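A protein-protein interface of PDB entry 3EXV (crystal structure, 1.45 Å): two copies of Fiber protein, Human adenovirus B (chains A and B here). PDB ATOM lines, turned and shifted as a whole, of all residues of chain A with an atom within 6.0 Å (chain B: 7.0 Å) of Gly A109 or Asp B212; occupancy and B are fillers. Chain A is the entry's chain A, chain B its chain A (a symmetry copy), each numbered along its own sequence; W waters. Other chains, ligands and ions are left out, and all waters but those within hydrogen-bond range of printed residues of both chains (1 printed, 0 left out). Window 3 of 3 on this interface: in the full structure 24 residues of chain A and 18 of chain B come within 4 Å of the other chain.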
ATOM      1  N   ASN A  18      13.859  29.643 -19.643  1.00  0.00           N
ATOM      2  CA  ASN A  18      12.629  28.860 -19.472  1.00  0.00           C
ATOM      3  C   ASN A  18      11.738  28.847 -20.715  1.00  0.00           C
ATOM      4  O   ASN A  18      11.022  27.874 -20.958  1.00  0.00           O
ATOM      5  CB  ASN A  18      11.825  29.387 -18.281  1.00  0.00           C
ATOM      6  CG  ASN A  18      12.464  29.050 -16.948  1.00  0.00           C
ATOM      7  OD1 ASN A  18      12.928  27.930 -16.732  1.00  0.00           O
ATOM      8  ND2 ASN A  18      12.481  30.019 -16.039  1.00  0.00           N
ATOM      9  N   TRP A  23       7.125  21.897 -22.923  1.00  0.00           N
ATOM     10  CA  TRP A  23       7.056  20.543 -22.373  1.00  0.00           C
ATOM     11  C   TRP A  23       5.797  20.230 -21.564  1.00  0.00           C
ATOM     12  O   TRP A  23       4.944  21.094 -21.344  1.00  0.00           O
ATOM     13  CB  TRP A  23       8.323  20.255 -21.540  1.00  0.00           C
ATOM     14  CG  TRP A  23       8.368  20.875 -20.151  1.00  0.00           C
ATOM     15  CD1 TRP A  23       7.627  21.924 -19.681  1.00  0.00           C
ATOM     16  CD2 TRP A  23       9.246  20.498 -19.084  1.00  0.00           C
ATOM     17  NE1 TRP A  23       7.970  22.202 -18.379  1.00  0.00           N
ATOM     18  CE2 TRP A  23       8.968  21.346 -17.991  1.00  0.00           C
ATOM     19  CE3 TRP A  23      10.237  19.520 -18.945  1.00  0.00           C
ATOM     20  CZ2 TRP A  23       9.644  21.241 -16.774  1.00  0.00           C
ATOM     21  CZ3 TRP A  23      10.907  19.417 -17.735  1.00  0.00           C
ATOM     22  CH2 TRP A  23      10.609  20.272 -16.667  1.00  0.00           C
ATOM     23  N   LYS A 107       8.971  25.923 -19.224  1.00  0.00           N
ATOM     24  CA  LYS A 107       9.535  25.363 -18.005  1.00  0.00           C
ATOM     25  C   LYS A 107       9.305  26.292 -16.819  1.00  0.00           C
ATOM     26  O   LYS A 107       9.550  27.493 -16.904  1.00  0.00           O
ATOM     27  CB  LYS A 107      11.037  25.111 -18.184  1.00  0.00           C
ATOM     28  CG  LYS A 107      11.757  24.622 -16.929  1.00  0.00           C
ATOM     29  CD  LYS A 107      13.229  24.370 -17.208  1.00  0.00           C
ATOM     30  CE  LYS A 107      14.034  24.244 -15.929  1.00  0.00           C
ATOM     31  NZ  LYS A 107      13.581  23.111 -15.086  1.00  0.00           N
ATOM     32  N   SER A 108       8.808  25.726 -15.724  1.00  0.00           N
ATOM     33  CA  SER A 108       8.751  26.419 -14.443  1.00  0.00           C
ATOM     34  C   SER A 108       9.131  25.408 -13.376  1.00  0.00           C
ATOM     35  O   SER A 108       8.292  24.642 -12.905  1.00  0.00           O
ATOM     36  CB  SER A 108       7.359  26.989 -14.185  1.00  0.00           C
ATOM     37  OG  SER A 108       7.320  27.680 -12.946  1.00  0.00           O
ATOM     38  N   GLY A 109      10.410  25.385 -13.020  1.00  0.00           N
ATOM     39  CA  GLY A 109      10.935  24.317 -12.187  1.00  0.00           C
ATOM     40  C   GLY A 109      10.768  22.987 -12.907  1.00  0.00           C
ATOM     41  O   GLY A 109      11.111  22.866 -14.085  1.00  0.00           O
ATOM     42  N   GLN A 110      10.205  22.001 -12.212  1.00  0.00           N
ATOM     43  CA  GLN A 110       9.946  20.683 -12.800  1.00  0.00           C
ATOM     44  C   GLN A 110       8.530  20.597 -13.377  1.00  0.00           C
ATOM     45  O   GLN A 110       8.081  19.519 -13.769  1.00  0.00           O
ATOM     46  CB  GLN A 110      10.127  19.592 -11.744  1.00  0.00           C
ATOM     47  CG  GLN A 110      11.488  19.608 -11.066  1.00  0.00           C
ATOM     48  CD  GLN A 110      12.609  19.183 -11.993  1.00  0.00           C
ATOM     49  OE1 GLN A 110      13.549  19.942 -12.244  1.00  0.00           O
ATOM     50  NE2 GLN A 110      12.512  17.968 -12.514  1.00  0.00           N
ATOM     51  N   ASN A 111       7.840  21.737 -13.435  1.00  0.00           N
ATOM     52  CA  ASN A 111       6.446  21.790 -13.855  1.00  0.00           C
ATOM     53  C   ASN A 111       6.249  22.687 -15.067  1.00  0.00           C
ATOM     54  O   ASN A 111       7.197  23.301 -15.558  1.00  0.00           O
ATOM     55  CB  ASN A 111       5.578  22.306 -12.699  1.00  0.00           C
ATOM     56  CG  ASN A 111       5.526  21.342 -11.530  1.00  0.00           C
ATOM     57  OD1 ASN A 111       5.901  20.175 -11.651  1.00  0.00           O
ATOM     58  ND2 ASN A 111       5.040  21.824 -10.391  1.00  0.00           N
ATOM     59  N   ALA B  55      15.368  22.483 -20.468  1.00  0.00           N
ATOM     60  CA  ALA B  55      15.041  21.676 -19.293  1.00  0.00           C
ATOM     61  C   ALA B  55      15.898  20.409 -19.185  1.00  0.00           C
ATOM     62  O   ALA B  55      15.795  19.672 -18.202  1.00  0.00           O
ATOM     63  CB  ALA B  55      13.567  21.300 -19.322  1.00  0.00           C
ATOM     64  N   ASN B 119      26.574  26.418 -10.178  1.00  0.00           N
ATOM     65  CA  ASN B 119      25.327  26.295 -10.908  1.00  0.00           C
ATOM     66  C   ASN B 119      25.269  24.788 -11.231  1.00  0.00           C
ATOM     67  O   ASN B 119      24.516  24.343 -12.090  1.00  0.00           O
ATOM     68  CB  ASN B 119      25.299  27.145 -12.183  1.00  0.00           C
ATOM     69  CG  ASN B 119      26.404  26.785 -13.155  1.00  0.00           C
ATOM     70  OD1 ASN B 119      27.472  26.328 -12.751  1.00  0.00           O
ATOM     71  ND2 ASN B 119      26.156  27.002 -14.444  1.00  0.00           N
ATOM     72  N   LYS B 121      24.366  22.195  -9.347  1.00  0.00           N
ATOM     73  CA  LYS B 121      23.129  21.507  -8.997  1.00  0.00           C
ATOM     74  C   LYS B 121      22.222  21.446 -10.228  1.00  0.00           C
ATOM     75  O   LYS B 121      21.520  20.462 -10.437  1.00  0.00           O
ATOM     76  CB  LYS B 121      22.415  22.208  -7.835  1.00  0.00           C
ATOM     77  CG  LYS B 121      21.301  21.380  -7.198  1.00  0.00           C
ATOM     78  CD  LYS B 121      20.671  22.109  -6.020  1.00  0.00           C
ATOM     79  CE  LYS B 121      19.579  21.280  -5.363  1.00  0.00           C
ATOM     80  NZ  LYS B 121      20.126  20.230  -4.461  1.00  0.00           N
ATOM     81  N   GLY B 122      22.283  22.490 -11.056  1.00  0.00           N
ATOM     82  CA  GLY B 122      21.510  22.556 -12.294  1.00  0.00           C
ATOM     83  C   GLY B 122      21.933  21.574 -13.379  1.00  0.00           C
ATOM     84  O   GLY B 122      21.245  21.433 -14.385  1.00  0.00           O
ATOM     85  N   PHE B 123      23.078  20.915 -13.192  1.00  0.00           N
ATOM     86  CA  PHE B 123      23.540  19.880 -14.130  1.00  0.00           C
ATOM     87  C   PHE B 123      23.147  18.473 -13.674  1.00  0.00           C
ATOM     88  O   PHE B 123      23.389  17.497 -14.383  1.00  0.00           O
ATOM     89  CB  PHE B 123      25.063  19.936 -14.286  1.00  0.00           C
ATOM     90  CG  PHE B 123      25.559  21.144 -15.020  1.00  0.00           C
ATOM     91  CD1 PHE B 123      25.811  22.326 -14.345  1.00  0.00           C
ATOM     92  CD2 PHE B 123      25.811  21.089 -16.385  1.00  0.00           C
ATOM     93  CE1 PHE B 123      26.287  23.443 -15.016  1.00  0.00           C
ATOM     94  CE2 PHE B 123      26.286  22.199 -17.064  1.00  0.00           C
ATOM     95  CZ  PHE B 123      26.523  23.378 -16.378  1.00  0.00           C
ATOM     96  N   MET B 124      22.561  18.366 -12.486  1.00  0.00           N
ATOM     97  CA  MET B 124      22.286  17.061 -11.884  1.00  0.00           C
ATOM     98  C   MET B 124      21.016  16.433 -12.442  1.00  0.00           C
ATOM     99  O   MET B 124      20.122  17.144 -12.911  1.00  0.00           O
ATOM    100  CB  MET B 124      22.148  17.196 -10.369  1.00  0.00           C
ATOM    101  CG  MET B 124      23.413  17.638  -9.653  1.00  0.00           C
ATOM    102  SD  MET B 124      24.750  16.437  -9.783  1.00  0.00           S
ATOM    103  CE  MET B 124      25.690  17.125 -11.145  1.00  0.00           C
ATOM    104  N   SER B 126      17.417  15.139 -12.323  1.00  0.00           N
ATOM    105  CA  SER B 126      16.269  15.512 -11.497  1.00  0.00           C
ATOM    106  C   SER B 126      15.834  14.385 -10.566  1.00  0.00           C
ATOM    107  O   SER B 126      15.638  13.253 -11.001  1.00  0.00           O
ATOM    108  CB  SER B 126      15.089  15.916 -12.384  1.00  0.00           C
ATOM    109  OG  SER B 126      13.892  15.986 -11.633  1.00  0.00           O
ATOM    110  N   TYR B 176      22.889  12.808  -5.570  1.00  0.00           N
ATOM    111  CA  TYR B 176      22.664  12.492  -6.985  1.00  0.00           C
ATOM    112  C   TYR B 176      23.613  11.397  -7.445  1.00  0.00           C
ATOM    113  O   TYR B 176      24.743  11.304  -6.966  1.00  0.00           O
ATOM    114  CB  TYR B 176      22.862  13.733  -7.858  1.00  0.00           C
ATOM    115  CG  TYR B 176      22.044  14.922  -7.423  1.00  0.00           C
ATOM    116  CD1 TYR B 176      22.582  15.887  -6.578  1.00  0.00           C
ATOM    117  CD2 TYR B 176      20.729  15.075  -7.844  1.00  0.00           C
ATOM    118  CE1 TYR B 176      21.830  16.977  -6.166  1.00  0.00           C
ATOM    119  CE2 TYR B 176      19.970  16.159  -7.442  1.00  0.00           C
ATOM    120  CZ  TYR B 176      20.525  17.108  -6.604  1.00  0.00           C
ATOM    121  OH  TYR B 176      19.773  18.186  -6.199  1.00  0.00           O
ATOM    122  N   ILE B 209      16.318  14.936 -17.823  1.00  0.00           N
ATOM    123  CA  ILE B 209      15.685  16.105 -17.238  1.00  0.00           C
ATOM    124  C   ILE B 209      16.521  16.549 -16.049  1.00  0.00           C
ATOM    125  O   ILE B 209      16.824  15.750 -15.162  1.00  0.00           O
ATOM    126  CB  ILE B 209      14.246  15.790 -16.790  1.00  0.00           C
ATOM    127  CG1 ILE B 209      13.372  15.490 -18.010  1.00  0.00           C
ATOM    128  CG2 ILE B 209      13.666  16.950 -15.994  1.00  0.00           C
ATOM    129  CD1 ILE B 209      12.041  14.869 -17.670  1.00  0.00           C
ATOM    130  N   ARG B 210      16.906  17.819 -16.039  1.00  0.00           N
ATOM    131  CA  ARG B 210      17.864  18.307 -15.054  1.00  0.00           C
ATOM    132  C   ARG B 210      17.196  18.878 -13.806  1.00  0.00           C
ATOM    133  O   ARG B 210      16.086  19.421 -13.858  1.00  0.00           O
ATOM    134  CB  ARG B 210      18.801  19.349 -15.681  1.00  0.00           C
ATOM    135  CG  ARG B 210      18.161  20.698 -15.973  1.00  0.00           C
ATOM    136  CD  ARG B 210      19.073  21.562 -16.832  1.00  0.00           C
ATOM    137  NE  ARG B 210      18.551  22.916 -17.005  1.00  0.00           N
ATOM    138  CZ  ARG B 210      18.609  23.878 -16.086  1.00  0.00           C
ATOM    139  NH1 ARG B 210      19.164  23.656 -14.900  1.00  0.00           N
ATOM    140  NH2 ARG B 210      18.099  25.074 -16.353  1.00  0.00           N
ATOM    141  N   GLU B 211      17.886  18.719 -12.682  1.00  0.00           N
ATOM    142  CA  GLU B 211      17.519  19.365 -11.436  1.00  0.00           C
ATOM    143  C   GLU B 211      17.675  20.873 -11.612  1.00  0.00           C
ATOM    144  O   GLU B 211      18.479  21.326 -12.423  1.00  0.00           O
ATOM    145  CB  GLU B 211      18.444  18.869 -10.320  1.00  0.00           C
ATOM    146  CG  GLU B 211      18.047  19.279  -8.913  1.00  0.00           C
ATOM    147  CD  GLU B 211      17.126  18.278  -8.240  1.00  0.00           C
ATOM    148  OE1 GLU B 211      16.268  17.689  -8.929  1.00  0.00           O
ATOM    149  OE2 GLU B 211      17.258  18.083  -7.015  1.00  0.00           O
ATOM    150  N   ASP B 212      16.889  21.647 -10.875  1.00  0.00           N
ATOM    151  CA  ASP B 212      17.036  23.100 -10.877  1.00  0.00           C
ATOM    152  C   ASP B 212      18.048  23.520  -9.814  1.00  0.00           C
ATOM    153  O   ASP B 212      18.273  22.800  -8.842  1.00  0.00           O
ATOM    154  CB  ASP B 212      15.688  23.773 -10.647  1.00  0.00           C
ATOM    155  CG  ASP B 212      14.733  23.558 -11.802  1.00  0.00           C
ATOM    156  OD1 ASP B 212      13.705  22.880 -11.606  1.00  0.00           O
ATOM    157  OD2 ASP B 212      15.033  24.037 -12.918  1.00  0.00           O
ATOM    158  N   ASP B 213      18.653  24.689 -10.009  1.00  0.00           N
ATOM    159  CA  ASP B 213      19.757  25.155  -9.155  1.00  0.00           C
ATOM    160  C   ASP B 213      19.359  25.354  -7.694  1.00  0.00           C
ATOM    161  O   ASP B 213      18.186  25.349  -7.335  1.00  0.00           O
ATOM    162  CB  ASP B 213      20.343  26.455  -9.713  1.00  0.00           C
ATOM    163  CG  ASP B 213      21.182  26.228 -10.951  1.00  0.00           C
ATOM    164  OD1 ASP B 213      22.145  25.438 -10.876  1.00  0.00           O
ATOM    165  OD2 ASP B 213      20.889  26.847 -11.995  1.00  0.00           O
ATOM    166  OXT ASP B 213      20.222  25.522  -6.829  1.00  0.00           O
HETATM  167  O   HOH W   1      14.487  20.581 -15.874  1.00  0.00           O
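NZ of Lys A107 is in salt-bridge range of OD2 of Asp B212.
The side-chain amide nitrogen (NE2) of Gln A110 lies within hydrogen-bond range of the side-chain hydroxyl (OG) of Ser B126, at 2.6 Å.
The backbone carbonyl oxygen of Arg B210 sits close to the side-chain amide oxygen of Gln A110 (3.1 Å).
The side-chain carboxylate of Asp B212 sits close to the side-chain amide oxygen of Gln A110, 3.0 Å away.
The backbone NH (N) of Lys A107 lies within hydrogen-bond range of the backbone carbonyl oxygen (O) of Asn A18.
The indole nitrogen (NE1) of Trp A23 is in hydrogen-bond range of the backbone carbonyl oxygen (O) of Asn A111, at 3.1 Å.
The side-chain amino group of Lys A107 is in hydrogen-bond range of the backbone carbonyl oxygen of Gly A109.
The backbone carbonyl oxygen of Ala B55 lies within hydrogen-bond range of the backbone NH of Arg B210 (3.1 Å).
The guanidinium group (NH1) of Arg B210 sits at hydrogen-bond distance from the backbone carbonyl oxygen (O) of Gly B122 (3.1 Å).
N of Ser B126 is in hydrogen-bond range of O of Ile B209, at 3.0 Å.
Printed residues of chain B within 4 Å of Trp A23: Ala B55.
Gly A109 touches just one residue of chain B: Asp B212 (3.2 Å).
Printed residues of chain B within 4 Å of Gln A110: Ser B126 (2.6 Å), Ile B209 (3.8 Å), Arg B210 (3.1 Å) and Asp B212 (3.0 Å).
Asn B119 touches none of the printed residues of chain A.
Gly B122 touches none of the printed residues of chain A.
Asp B212 touches three residues of chain A.
The nearest residue of chain A that does not touch Asp B212 is Ser A108 (5.5 Å).
The nearest printed residue of chain B that does not touch Lys A107 is Arg B210 (4.2 Å).
Printed residues of chain B that touch a printed residue of chain A: Ala B55, Ser B126, Ile B209, Arg B210 and Asp B212.
Among the printed residues, Asp or Glu carboxylates within 4 Å of a Lys or Arg side-chain nitrogen of the other chain: Lys A107 with Asp B212.
Water W1 lies within hydrogen-bond range of the side-chain amino group of Lys A107 (2.8 Å), the backbone carbonyl oxygen of Ala B55 (2.8 Å) and the backbone carbonyl oxygen of Arg B210 (2.8 Å).
Among the printed residues, merely in contact across the chains: Trp A23 with Ala B55 (3.6 Å), Lys A107 with Ala B55 (3.7 Å), Gly A109 with Asp B212 (3.2 Å) and Gln A110 with Ile B209 (3.8 Å).
No position is printed for both chains.
Of the 8 pairs that touch across the chains among the printed residues, none has its exchanged pair printed and touching as well.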
